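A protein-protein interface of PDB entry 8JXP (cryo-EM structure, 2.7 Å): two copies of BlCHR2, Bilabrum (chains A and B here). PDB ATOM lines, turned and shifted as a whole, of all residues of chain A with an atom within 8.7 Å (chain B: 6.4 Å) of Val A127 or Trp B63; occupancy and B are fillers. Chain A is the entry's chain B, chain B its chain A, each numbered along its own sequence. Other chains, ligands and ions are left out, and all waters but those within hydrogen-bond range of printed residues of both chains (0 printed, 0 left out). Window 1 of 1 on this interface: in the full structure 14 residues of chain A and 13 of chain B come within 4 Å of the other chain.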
ATOM      1  N   VAL A 113     -27.277  34.423 -23.033  1.00  0.00           N
ATOM      2  CA  VAL A 113     -26.479  33.211 -22.969  1.00  0.00           C
ATOM      3  C   VAL A 113     -27.403  32.013 -22.967  1.00  0.00           C
ATOM      4  O   VAL A 113     -27.133  31.030 -23.639  1.00  0.00           O
ATOM      5  CB  VAL A 113     -25.554  33.193 -21.744  1.00  0.00           C
ATOM      6  CG1 VAL A 113     -24.559  32.050 -21.845  1.00  0.00           C
ATOM      7  CG2 VAL A 113     -24.796  34.499 -21.661  1.00  0.00           C
ATOM      8  N   LEU A 114     -28.513  32.091 -22.248  1.00  0.00           N
ATOM      9  CA  LEU A 114     -29.482  31.004 -22.273  1.00  0.00           C
ATOM     10  C   LEU A 114     -29.962  30.783 -23.693  1.00  0.00           C
ATOM     11  O   LEU A 114     -29.970  29.660 -24.158  1.00  0.00           O
ATOM     12  CB  LEU A 114     -30.665  31.304 -21.367  1.00  0.00           C
ATOM     13  CG  LEU A 114     -30.901  30.349 -20.200  1.00  0.00           C
ATOM     14  CD1 LEU A 114     -32.391  30.172 -19.967  1.00  0.00           C
ATOM     15  CD2 LEU A 114     -30.228  29.008 -20.435  1.00  0.00           C
ATOM     16  N   CYS A 117     -27.307  29.077 -25.769  1.00  0.00           N
ATOM     17  CA  CYS A 117     -27.191  27.692 -25.351  1.00  0.00           C
ATOM     18  C   CYS A 117     -28.375  26.801 -25.690  1.00  0.00           C
ATOM     19  O   CYS A 117     -28.211  25.609 -25.847  1.00  0.00           O
ATOM     20  CB  CYS A 117     -26.899  27.633 -23.859  1.00  0.00           C
ATOM     21  SG  CYS A 117     -25.259  28.224 -23.398  1.00  0.00           S
ATOM     22  N   LEU A 122     -26.049  24.036 -26.805  1.00  0.00           N
ATOM     23  CA  LEU A 122     -24.774  23.982 -26.123  1.00  0.00           C
ATOM     24  C   LEU A 122     -25.061  23.389 -24.768  1.00  0.00           C
ATOM     25  O   LEU A 122     -26.112  23.642 -24.189  1.00  0.00           O
ATOM     26  CB  LEU A 122     -24.198  25.384 -25.956  1.00  0.00           C
ATOM     27  CG  LEU A 122     -23.220  25.937 -26.990  1.00  0.00           C
ATOM     28  CD1 LEU A 122     -23.113  25.021 -28.194  1.00  0.00           C
ATOM     29  CD2 LEU A 122     -23.644  27.335 -27.402  1.00  0.00           C
ATOM     30  N   ARG A 123     -24.135  22.599 -24.248  1.00  0.00           N
ATOM     31  CA  ARG A 123     -24.339  21.969 -22.959  1.00  0.00           C
ATOM     32  C   ARG A 123     -24.177  22.960 -21.824  1.00  0.00           C
ATOM     33  O   ARG A 123     -23.795  24.105 -22.055  1.00  0.00           O
ATOM     34  CB  ARG A 123     -23.374  20.801 -22.778  1.00  0.00           C
ATOM     35  CG  ARG A 123     -23.544  19.696 -23.805  1.00  0.00           C
ATOM     36  CD  ARG A 123     -22.204  19.297 -24.395  1.00  0.00           C
ATOM     37  NE  ARG A 123     -21.375  18.589 -23.426  1.00  0.00           N
ATOM     38  CZ  ARG A 123     -20.096  18.295 -23.616  1.00  0.00           C
ATOM     39  NH1 ARG A 123     -19.494  18.652 -24.743  1.00  0.00           N
ATOM     40  NH2 ARG A 123     -19.415  17.646 -22.681  1.00  0.00           N
ATOM     41  N   TYR A 124     -24.464  22.528 -20.600  1.00  0.00           N
ATOM     42  CA  TYR A 124     -24.329  23.394 -19.431  1.00  0.00           C
ATOM     43  C   TYR A 124     -25.030  24.727 -19.626  1.00  0.00           C
ATOM     44  O   TYR A 124     -24.496  25.765 -19.252  1.00  0.00           O
ATOM     45  CB  TYR A 124     -22.855  23.622 -19.076  1.00  0.00           C
ATOM     46  CG  TYR A 124     -21.945  22.451 -19.364  1.00  0.00           C
ATOM     47  CD1 TYR A 124     -22.165  21.210 -18.781  1.00  0.00           C
ATOM     48  CD2 TYR A 124     -20.858  22.590 -20.216  1.00  0.00           C
ATOM     49  CE1 TYR A 124     -21.333  20.139 -19.046  1.00  0.00           C
ATOM     50  CE2 TYR A 124     -20.022  21.526 -20.484  1.00  0.00           C
ATOM     51  CZ  TYR A 124     -20.264  20.305 -19.898  1.00  0.00           C
ATOM     52  OH  TYR A 124     -19.430  19.245 -20.163  1.00  0.00           O
ATOM     53  N   LYS A 125     -26.226  24.704 -20.204  1.00  0.00           N
ATOM     54  CA  LYS A 125     -26.951  25.938 -20.468  1.00  0.00           C
ATOM     55  C   LYS A 125     -27.115  26.786 -19.233  1.00  0.00           C
ATOM     56  O   LYS A 125     -26.781  27.969 -19.233  1.00  0.00           O
ATOM     57  CB  LYS A 125     -28.331  25.617 -21.038  1.00  0.00           C
ATOM     58  CG  LYS A 125     -28.416  24.274 -21.739  1.00  0.00           C
ATOM     59  CD  LYS A 125     -29.493  24.288 -22.808  1.00  0.00           C
ATOM     60  CE  LYS A 125     -29.432  23.033 -23.666  1.00  0.00           C
ATOM     61  NZ  LYS A 125     -30.115  23.221 -24.975  1.00  0.00           N
ATOM     62  N   LEU A 126     -27.659  26.182 -18.183  1.00  0.00           N
ATOM     63  CA  LEU A 126     -27.911  26.920 -16.957  1.00  0.00           C
ATOM     64  C   LEU A 126     -26.618  27.331 -16.305  1.00  0.00           C
ATOM     65  O   LEU A 126     -26.506  28.451 -15.855  1.00  0.00           O
ATOM     66  CB  LEU A 126     -28.768  26.106 -15.994  1.00  0.00           C
ATOM     67  CG  LEU A 126     -30.254  26.474 -15.980  1.00  0.00           C
ATOM     68  CD1 LEU A 126     -30.443  27.961 -16.241  1.00  0.00           C
ATOM     69  CD2 LEU A 126     -31.022  25.650 -16.998  1.00  0.00           C
ATOM     70  N   VAL A 127     -25.633  26.443 -16.272  1.00  0.00           N
ATOM     71  CA  VAL A 127     -24.333  26.798 -15.720  1.00  0.00           C
ATOM     72  C   VAL A 127     -23.826  28.081 -16.352  1.00  0.00           C
ATOM     73  O   VAL A 127     -23.588  29.052 -15.651  1.00  0.00           O
ATOM     74  CB  VAL A 127     -23.296  25.682 -15.932  1.00  0.00           C
ATOM     75  CG1 VAL A 127     -21.959  26.065 -15.317  1.00  0.00           C
ATOM     76  CG2 VAL A 127     -23.804  24.375 -15.347  1.00  0.00           C
ATOM     77  N   PHE A 128     -23.684  28.098 -17.672  1.00  0.00           N
ATOM     78  CA  PHE A 128     -23.210  29.288 -18.374  1.00  0.00           C
ATOM     79  C   PHE A 128     -24.029  30.521 -18.039  1.00  0.00           C
ATOM     80  O   PHE A 128     -23.473  31.569 -17.723  1.00  0.00           O
ATOM     81  CB  PHE A 128     -23.248  29.061 -19.883  1.00  0.00           C
ATOM     82  CG  PHE A 128     -22.104  28.243 -20.405  1.00  0.00           C
ATOM     83  CD1 PHE A 128     -20.802  28.566 -20.082  1.00  0.00           C
ATOM     84  CD2 PHE A 128     -22.337  27.155 -21.225  1.00  0.00           C
ATOM     85  CE1 PHE A 128     -19.751  27.814 -20.563  1.00  0.00           C
ATOM     86  CE2 PHE A 128     -21.291  26.397 -21.709  1.00  0.00           C
ATOM     87  CZ  PHE A 128     -19.995  26.726 -21.378  1.00  0.00           C
ATOM     88  N   SER A 129     -25.349  30.402 -18.093  1.00  0.00           N
ATOM     89  CA  SER A 129     -26.206  31.554 -17.851  1.00  0.00           C
ATOM     90  C   SER A 129     -26.061  32.128 -16.452  1.00  0.00           C
ATOM     91  O   SER A 129     -26.117  33.338 -16.275  1.00  0.00           O
ATOM     92  CB  SER A 129     -27.663  31.192 -18.119  1.00  0.00           C
ATOM     93  OG  SER A 129     -28.351  30.907 -16.917  1.00  0.00           O
ATOM     94  N   SER A 130     -25.868  31.269 -15.459  1.00  0.00           N
ATOM     95  CA  SER A 130     -25.736  31.729 -14.082  1.00  0.00           C
ATOM     96  C   SER A 130     -24.352  32.300 -13.861  1.00  0.00           C
ATOM     97  O   SER A 130     -24.171  33.240 -13.082  1.00  0.00           O
ATOM     98  CB  SER A 130     -26.002  30.584 -13.113  1.00  0.00           C
ATOM     99  OG  SER A 130     -25.011  29.580 -13.225  1.00  0.00           O
ATOM    100  N   SER A 131     -23.367  31.742 -14.546  1.00  0.00           N
ATOM    101  CA  SER A 131     -22.025  32.263 -14.435  1.00  0.00           C
ATOM    102  C   SER A 131     -22.040  33.690 -14.940  1.00  0.00           C
ATOM    103  O   SER A 131     -21.485  34.577 -14.304  1.00  0.00           O
ATOM    104  CB  SER A 131     -21.054  31.421 -15.256  1.00  0.00           C
ATOM    105  OG  SER A 131     -20.332  32.222 -16.172  1.00  0.00           O
ATOM    106  N   ILE A 132     -22.692  33.923 -16.074  1.00  0.00           N
ATOM    107  CA  ILE A 132     -22.695  35.263 -16.643  1.00  0.00           C
ATOM    108  C   ILE A 132     -23.458  36.225 -15.743  1.00  0.00           C
ATOM    109  O   ILE A 132     -23.027  37.354 -15.553  1.00  0.00           O
ATOM    110  CB  ILE A 132     -23.168  35.261 -18.114  1.00  0.00           C
ATOM    111  CG1 ILE A 132     -21.959  35.373 -19.044  1.00  0.00           C
ATOM    112  CG2 ILE A 132     -24.126  36.395 -18.415  1.00  0.00           C
ATOM    113  CD1 ILE A 132     -21.342  34.045 -19.425  1.00  0.00           C
ATOM    114  N   ALA A 133     -24.543  35.772 -15.126  1.00  0.00           N
ATOM    115  CA  ALA A 133     -25.264  36.621 -14.186  1.00  0.00           C
ATOM    116  C   ALA A 133     -24.366  37.022 -13.032  1.00  0.00           C
ATOM    117  O   ALA A 133     -24.368  38.171 -12.613  1.00  0.00           O
ATOM    118  CB  ALA A 133     -26.493  35.911 -13.666  1.00  0.00           C
ATOM    119  N   CYS A 134     -23.584  36.081 -12.521  1.00  0.00           N
ATOM    120  CA  CYS A 134     -22.677  36.373 -11.419  1.00  0.00           C
ATOM    121  C   CYS A 134     -21.529  37.281 -11.818  1.00  0.00           C
ATOM    122  O   CYS A 134     -21.093  38.102 -11.027  1.00  0.00           O
ATOM    123  CB  CYS A 134     -22.124  35.081 -10.825  1.00  0.00           C
ATOM    124  SG  CYS A 134     -23.354  34.086  -9.952  1.00  0.00           S
ATOM    125  N   LEU A 135     -21.041  37.151 -13.046  1.00  0.00           N
ATOM    126  CA  LEU A 135     -19.944  37.990 -13.518  1.00  0.00           C
ATOM    127  C   LEU A 135     -20.431  39.375 -13.849  1.00  0.00           C
ATOM    128  O   LEU A 135     -19.652  40.318 -13.880  1.00  0.00           O
ATOM    129  CB  LEU A 135     -19.288  37.385 -14.749  1.00  0.00           C
ATOM    130  CG  LEU A 135     -18.658  36.020 -14.535  1.00  0.00           C
ATOM    131  CD1 LEU A 135     -18.403  35.346 -15.872  1.00  0.00           C
ATOM    132  CD2 LEU A 135     -17.401  36.137 -13.696  1.00  0.00           C
ATOM    133  N   ALA A 164     -15.234  31.422 -18.543  1.00  0.00           N
ATOM    134  CA  ALA A 164     -16.520  31.114 -19.159  1.00  0.00           C
ATOM    135  C   ALA A 164     -16.446  31.283 -20.656  1.00  0.00           C
ATOM    136  O   ALA A 164     -17.103  30.563 -21.389  1.00  0.00           O
ATOM    137  CB  ALA A 164     -17.610  31.997 -18.587  1.00  0.00           C
ATOM    138  N   ALA A 167     -14.694  28.164 -21.996  1.00  0.00           N
ATOM    139  CA  ALA A 167     -15.626  27.053 -21.957  1.00  0.00           C
ATOM    140  C   ALA A 167     -16.694  27.180 -23.034  1.00  0.00           C
ATOM    141  O   ALA A 167     -17.051  26.192 -23.666  1.00  0.00           O
ATOM    142  CB  ALA A 167     -16.255  26.944 -20.586  1.00  0.00           C
ATOM    143  N   GLU A 171     -17.519  24.707 -26.242  1.00  0.00           N
ATOM    144  CA  GLU A 171     -18.850  24.167 -26.505  1.00  0.00           C
ATOM    145  C   GLU A 171     -19.338  24.404 -27.931  1.00  0.00           C
ATOM    146  O   GLU A 171     -19.829  23.485 -28.570  1.00  0.00           O
ATOM    147  CB  GLU A 171     -19.864  24.721 -25.509  1.00  0.00           C
ATOM    148  CG  GLU A 171     -20.507  23.663 -24.637  1.00  0.00           C
ATOM    149  CD  GLU A 171     -19.494  22.967 -23.759  1.00  0.00           C
ATOM    150  OE1 GLU A 171     -19.350  21.732 -23.877  1.00  0.00           O
ATOM    151  OE2 GLU A 171     -18.833  23.655 -22.954  1.00  0.00           O
ATOM    152  N   MET B  38     -15.066  19.387  -6.444  1.00  0.00           N
ATOM    153  CA  MET B  38     -16.352  18.810  -6.780  1.00  0.00           C
ATOM    154  C   MET B  38     -16.596  18.945  -8.268  1.00  0.00           C
ATOM    155  O   MET B  38     -17.086  18.018  -8.893  1.00  0.00           O
ATOM    156  CB  MET B  38     -17.462  19.499  -5.992  1.00  0.00           C
ATOM    157  CG  MET B  38     -17.881  18.784  -4.722  1.00  0.00           C
ATOM    158  SD  MET B  38     -17.815  19.819  -3.248  1.00  0.00           S
ATOM    159  CE  MET B  38     -19.134  20.978  -3.571  1.00  0.00           C
ATOM    160  N   ALA B  39     -16.239  20.089  -8.845  1.00  0.00           N
ATOM    161  CA  ALA B  39     -16.418  20.308 -10.277  1.00  0.00           C
ATOM    162  C   ALA B  39     -15.550  19.373 -11.074  1.00  0.00           C
ATOM    163  O   ALA B  39     -16.009  18.774 -12.034  1.00  0.00           O
ATOM    164  CB  ALA B  39     -16.122  21.745 -10.650  1.00  0.00           C
ATOM    165  N   TRP B  40     -14.293  19.233 -10.680  1.00  0.00           N
ATOM    166  CA  TRP B  40     -13.420  18.294 -11.354  1.00  0.00           C
ATOM    167  C   TRP B  40     -13.999  16.891 -11.262  1.00  0.00           C
ATOM    168  O   TRP B  40     -14.113  16.217 -12.264  1.00  0.00           O
ATOM    169  CB  TRP B  40     -12.011  18.332 -10.768  1.00  0.00           C
ATOM    170  CG  TRP B  40     -11.153  17.219 -11.252  1.00  0.00           C
ATOM    171  CD1 TRP B  40     -10.600  17.091 -12.490  1.00  0.00           C
ATOM    172  CD2 TRP B  40     -10.758  16.058 -10.513  1.00  0.00           C
ATOM    173  NE1 TRP B  40      -9.882  15.925 -12.568  1.00  0.00           N
ATOM    174  CE2 TRP B  40      -9.964  15.272 -11.367  1.00  0.00           C
ATOM    175  CE3 TRP B  40     -11.000  15.609  -9.215  1.00  0.00           C
ATOM    176  CZ2 TRP B  40      -9.407  14.065 -10.963  1.00  0.00           C
ATOM    177  CZ3 TRP B  40     -10.448  14.410  -8.817  1.00  0.00           C
ATOM    178  CH2 TRP B  40      -9.663  13.653  -9.686  1.00  0.00           C
ATOM    179  N   THR B  42     -17.026  15.819 -10.850  1.00  0.00           N
ATOM    180  CA  THR B  42     -18.225  15.637 -11.653  1.00  0.00           C
ATOM    181  C   THR B  42     -17.888  15.587 -13.129  1.00  0.00           C
ATOM    182  O   THR B  42     -18.443  14.781 -13.857  1.00  0.00           O
ATOM    183  CB  THR B  42     -19.296  16.713 -11.399  1.00  0.00           C
ATOM    184  OG1 THR B  42     -18.690  18.002 -11.342  1.00  0.00           O
ATOM    185  CG2 THR B  42     -20.015  16.439 -10.096  1.00  0.00           C
ATOM    186  N   ALA B  43     -16.974  16.438 -13.574  1.00  0.00           N
ATOM    187  CA  ALA B  43     -16.583  16.448 -14.976  1.00  0.00           C
ATOM    188  C   ALA B  43     -15.787  15.217 -15.348  1.00  0.00           C
ATOM    189  O   ALA B  43     -16.101  14.556 -16.335  1.00  0.00           O
ATOM    190  CB  ALA B  43     -15.785  17.696 -15.293  1.00  0.00           C
ATOM    191  N   ALA B  44     -14.759  14.901 -14.569  1.00  0.00           N
ATOM    192  CA  ALA B  44     -13.890  13.769 -14.873  1.00  0.00           C
ATOM    193  C   ALA B  44     -14.629  12.473 -15.133  1.00  0.00           C
ATOM    194  O   ALA B  44     -14.340  11.778 -16.105  1.00  0.00           O
ATOM    195  CB  ALA B  44     -12.871  13.574 -13.763  1.00  0.00           C
ATOM    196  N   PRO B  58     -21.766  15.445 -18.013  1.00  0.00           N
ATOM    197  CA  PRO B  58     -22.359  15.508 -16.675  1.00  0.00           C
ATOM    198  C   PRO B  58     -23.689  16.229 -16.699  1.00  0.00           C
ATOM    199  O   PRO B  58     -23.812  17.246 -17.377  1.00  0.00           O
ATOM    200  CB  PRO B  58     -21.337  16.319 -15.876  1.00  0.00           C
ATOM    201  CG  PRO B  58     -20.062  16.205 -16.640  1.00  0.00           C
ATOM    202  CD  PRO B  58     -20.464  16.124 -18.079  1.00  0.00           C
ATOM    203  N   PRO B  59     -24.686  15.706 -15.975  1.00  0.00           N
ATOM    204  CA  PRO B  59     -25.984  16.376 -15.898  1.00  0.00           C
ATOM    205  C   PRO B  59     -25.852  17.806 -15.389  1.00  0.00           C
ATOM    206  O   PRO B  59     -24.915  18.113 -14.660  1.00  0.00           O
ATOM    207  CB  PRO B  59     -26.761  15.516 -14.903  1.00  0.00           C
ATOM    208  CG  PRO B  59     -26.150  14.165 -15.023  1.00  0.00           C
ATOM    209  CD  PRO B  59     -24.696  14.390 -15.313  1.00  0.00           C
ATOM    210  N   GLU B  60     -26.783  18.677 -15.755  1.00  0.00           N
ATOM    211  CA  GLU B  60     -26.694  20.076 -15.353  1.00  0.00           C
ATOM    212  C   GLU B  60     -26.851  20.258 -13.857  1.00  0.00           C
ATOM    213  O   GLU B  60     -26.422  21.266 -13.304  1.00  0.00           O
ATOM    214  CB  GLU B  60     -27.736  20.910 -16.087  1.00  0.00           C
ATOM    215  CG  GLU B  60     -27.184  21.697 -17.261  1.00  0.00           C
ATOM    216  CD  GLU B  60     -28.194  21.852 -18.379  1.00  0.00           C
ATOM    217  OE1 GLU B  60     -29.309  22.340 -18.106  1.00  0.00           O
ATOM    218  OE2 GLU B  60     -27.874  21.481 -19.526  1.00  0.00           O
ATOM    219  N   GLU B  61     -27.469  19.290 -13.195  1.00  0.00           N
ATOM    220  CA  GLU B  61     -27.650  19.364 -11.755  1.00  0.00           C
ATOM    221  C   GLU B  61     -26.391  18.926 -11.031  1.00  0.00           C
ATOM    222  O   GLU B  61     -26.229  19.205  -9.846  1.00  0.00           O
ATOM    223  CB  GLU B  61     -28.833  18.505 -11.328  1.00  0.00           C
ATOM    224  CG  GLU B  61     -29.893  18.337 -12.403  1.00  0.00           C
ATOM    225  CD  GLU B  61     -29.866  16.958 -13.030  1.00  0.00           C
ATOM    226  OE1 GLU B  61     -30.043  16.862 -14.263  1.00  0.00           O
ATOM    227  OE2 GLU B  61     -29.666  15.973 -12.293  1.00  0.00           O
ATOM    228  N   ASN B  62     -25.500  18.233 -11.728  1.00  0.00           N
ATOM    229  CA  ASN B  62     -24.238  17.843 -11.119  1.00  0.00           C
ATOM    230  C   ASN B  62     -23.396  19.082 -10.892  1.00  0.00           C
ATOM    231  O   ASN B  62     -22.395  19.018 -10.193  1.00  0.00           O
ATOM    232  CB  ASN B  62     -23.501  16.838 -11.997  1.00  0.00           C
ATOM    233  CG  ASN B  62     -23.989  15.421 -11.790  1.00  0.00           C
ATOM    234  OD1 ASN B  62     -25.121  15.199 -11.367  1.00  0.00           O
ATOM    235  ND2 ASN B  62     -23.136  14.450 -12.092  1.00  0.00           N
ATOM    236  N   TRP B  63     -23.783  20.203 -11.492  1.00  0.00           N
ATOM    237  CA  TRP B  63     -23.088  21.471 -11.295  1.00  0.00           C
ATOM    238  C   TRP B  63     -23.706  22.371 -10.244  1.00  0.00           C
ATOM    239  O   TRP B  63     -23.088  23.345  -9.841  1.00  0.00           O
ATOM    240  CB  TRP B  63     -23.010  22.222 -12.618  1.00  0.00           C
ATOM    241  CG  TRP B  63     -22.402  21.429 -13.721  1.00  0.00           C
ATOM    242  CD1 TRP B  63     -23.033  20.961 -14.833  1.00  0.00           C
ATOM    243  CD2 TRP B  63     -21.038  21.011 -13.823  1.00  0.00           C
ATOM    244  NE1 TRP B  63     -22.145  20.274 -15.624  1.00  0.00           N
ATOM    245  CE2 TRP B  63     -20.914  20.291 -15.025  1.00  0.00           C
ATOM    246  CE3 TRP B  63     -19.910  21.175 -13.017  1.00  0.00           C
ATOM    247  CZ2 TRP B  63     -19.709  19.738 -15.439  1.00  0.00           C
ATOM    248  CZ3 TRP B  63     -18.717  20.627 -13.430  1.00  0.00           C
ATOM    249  CH2 TRP B  63     -18.624  19.914 -14.627  1.00  0.00           C
ATOM    250  N   LEU B  64     -24.922  22.071  -9.806  1.00  0.00           N
ATOM    251  CA  LEU B  64     -25.535  22.850  -8.745  1.00  0.00           C
ATOM    252  C   LEU B  64     -24.658  22.784  -7.512  1.00  0.00           C
ATOM    253  O   LEU B  64     -24.308  23.813  -6.960  1.00  0.00           O
ATOM    254  CB  LEU B  64     -26.935  22.331  -8.430  1.00  0.00           C
ATOM    255  CG  LEU B  64     -28.106  23.294  -8.609  1.00  0.00           C
ATOM    256  CD1 LEU B  64     -29.338  22.754  -7.903  1.00  0.00           C
ATOM    257  CD2 LEU B  64     -27.752  24.678  -8.087  1.00  0.00           C
ATOM    258  N   SER B  65     -24.225  21.598  -7.087  1.00  0.00           N
ATOM    259  CA  SER B  65     -23.390  21.461  -5.869  1.00  0.00           C
ATOM    260  C   SER B  65     -22.017  22.190  -5.948  1.00  0.00           C
ATOM    261  O   SER B  65     -21.768  23.041  -5.095  1.00  0.00           O
ATOM    262  CB  SER B  65     -23.259  19.999  -5.419  1.00  0.00           C
ATOM    263  OG  SER B  65     -23.573  19.860  -4.046  1.00  0.00           O
ATOM    264  N   PRO B  66     -21.106  21.854  -6.930  1.00  0.00           N
ATOM    265  CA  PRO B  66     -19.883  22.668  -7.008  1.00  0.00           C
ATOM    266  C   PRO B  66     -20.249  24.124  -7.127  1.00  0.00           C
ATOM    267  O   PRO B  66     -19.619  24.967  -6.489  1.00  0.00           O
ATOM    268  CB  PRO B  66     -19.259  22.227  -8.325  1.00  0.00           C
ATOM    269  CG  PRO B  66     -19.724  20.839  -8.522  1.00  0.00           C
ATOM    270  CD  PRO B  66     -21.115  20.819  -7.995  1.00  0.00           C
ATOM    271  N   GLY B  67     -21.259  24.418  -7.934  1.00  0.00           N
ATOM    272  CA  GLY B  67     -21.690  25.784  -8.141  1.00  0.00           C
ATOM    273  C   GLY B  67     -21.834  26.574  -6.873  1.00  0.00           C
ATOM    274  O   GLY B  67     -21.180  27.581  -6.738  1.00  0.00           O
ATOM    275  N   ILE B  68     -22.672  26.125  -5.950  1.00  0.00           N
ATOM    276  CA  ILE B  68     -22.902  26.853  -4.706  1.00  0.00           C
ATOM    277  C   ILE B  68     -21.607  27.105  -3.957  1.00  0.00           C
ATOM    278  O   ILE B  68     -21.328  28.228  -3.575  1.00  0.00           O
ATOM    279  CB  ILE B  68     -23.873  26.111  -3.776  1.00  0.00           C
ATOM    280  CG1 ILE B  68     -25.150  25.758  -4.521  1.00  0.00           C
ATOM    281  CG2 ILE B  68     -24.207  26.957  -2.558  1.00  0.00           C
ATOM    282  CD1 ILE B  68     -25.767  24.459  -4.062  1.00  0.00           C
ATOM    283  N   ASP B 115     -30.591  21.167  -4.513  1.00  0.00           N
ATOM    284  CA  ASP B 115     -29.632  20.085  -4.691  1.00  0.00           C
ATOM    285  C   ASP B 115     -30.071  18.838  -3.962  1.00  0.00           C
ATOM    286  O   ASP B 115     -30.224  17.790  -4.575  1.00  0.00           O
ATOM    287  CB  ASP B 115     -28.288  20.497  -4.133  1.00  0.00           C
ATOM    288  CG  ASP B 115     -27.214  20.509  -5.169  1.00  0.00           C
ATOM    289  OD1 ASP B 115     -27.171  19.586  -6.010  1.00  0.00           O
ATOM    290  OD2 ASP B 115     -26.409  21.453  -5.137  1.00  0.00           O
ATOM    291  N   ARG B 243     -23.684  11.093  -4.474  1.00  0.00           N
ATOM    292  CA  ARG B 243     -23.854  11.005  -5.919  1.00  0.00           C
ATOM    293  C   ARG B 243     -22.903  10.007  -6.521  1.00  0.00           C
ATOM    294  O   ARG B 243     -23.301   9.191  -7.338  1.00  0.00           O
ATOM    295  CB  ARG B 243     -23.562  12.368  -6.533  1.00  0.00           C
ATOM    296  CG  ARG B 243     -24.095  12.596  -7.930  1.00  0.00           C
ATOM    297  CD  ARG B 243     -24.478  14.054  -8.112  1.00  0.00           C
ATOM    298  NE  ARG B 243     -23.329  14.955  -8.062  1.00  0.00           N
ATOM    299  CZ  ARG B 243     -23.215  15.970  -7.209  1.00  0.00           C
ATOM    300  NH1 ARG B 243     -24.174  16.207  -6.326  1.00  0.00           N
ATOM    301  NH2 ARG B 243     -22.140  16.744  -7.233  1.00  0.00           N
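Of chain B, only Trp B63 comes within 4 Å of Val A127.
Of chain A, only Tyr A124 and Val A127 come within 4 Å of Trp B63.
Of the printed residues of chain B, Tyr A124 touches Pro B58, Glu B60 and Trp B63.
Of the printed residues of chain B, Lys A125 touches Glu B60 (3.6 Å).
Of the printed residues of chain A, Pro B58 touches Tyr A124 (3.9 Å).
Of the printed residues of chain B, Leu A126 touches Glu B60.
Leu A122 touches none of the printed residues of chain B.
Asp B115 touches none of the printed residues of chain A.
The nearest residue of chain B that does not touch Val A127 is Glu B60 (4.5 Å).
The nearest residue of chain A that does not touch Trp B63 is Arg A123 (7.1 Å).
Tyr A124 touches Pro B58.
Glu B60 touches Tyr A124.
Trp B63 touches Tyr A124 (NE1 to CD1, 3.3 Å).
Lys A125 touches Glu B60 (CG to OE2, 3.6 Å).
OE1 of Glu B60 touches CD2 of Leu A126, 3.9 Å away.
Val A127 touches Trp B63 (CG2 to CD1, 3.5 Å).
No position is printed for both chains.
Of the 6 pairs that touch across the chains among the printed residues, none has its exchanged pair printed and touching as well.
Of the 19 printed residues of chain B, 3 touch a printed residue of chain A.
Printed residues of chain B that touch a printed residue of chain A: Pro B58, Glu B60 and Trp B63.
Hydrophobic or aromatic side chains of chain B within 4 Å of the printed part of chain A: Pro B58 and Trp B63.
Among the printed residues, 6 pairs touch across the chains.
The backbone carbonyl oxygen (O) of Cys A117 is in hydrogen-bond range of the side-chain amino group (NZ) of Lys A125.
The guanidinium group of Arg A123 sits at hydrogen-bond distance from the side-chain hydroxyl of Tyr A124 (3.0 Å).
The side-chain hydroxyl of Ser A129 lies within hydrogen-bond range of the backbone carbonyl oxygen of Leu A126 (3.3 Å).
The side-chain hydroxyl (OG) of Ser A130 lies within hydrogen-bond range of the backbone carbonyl oxygen (O) of Leu A126, 3.2 Å away.
OG of Ser A130 sits at hydrogen-bond distance from O of Val A127 (2.9 Å).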
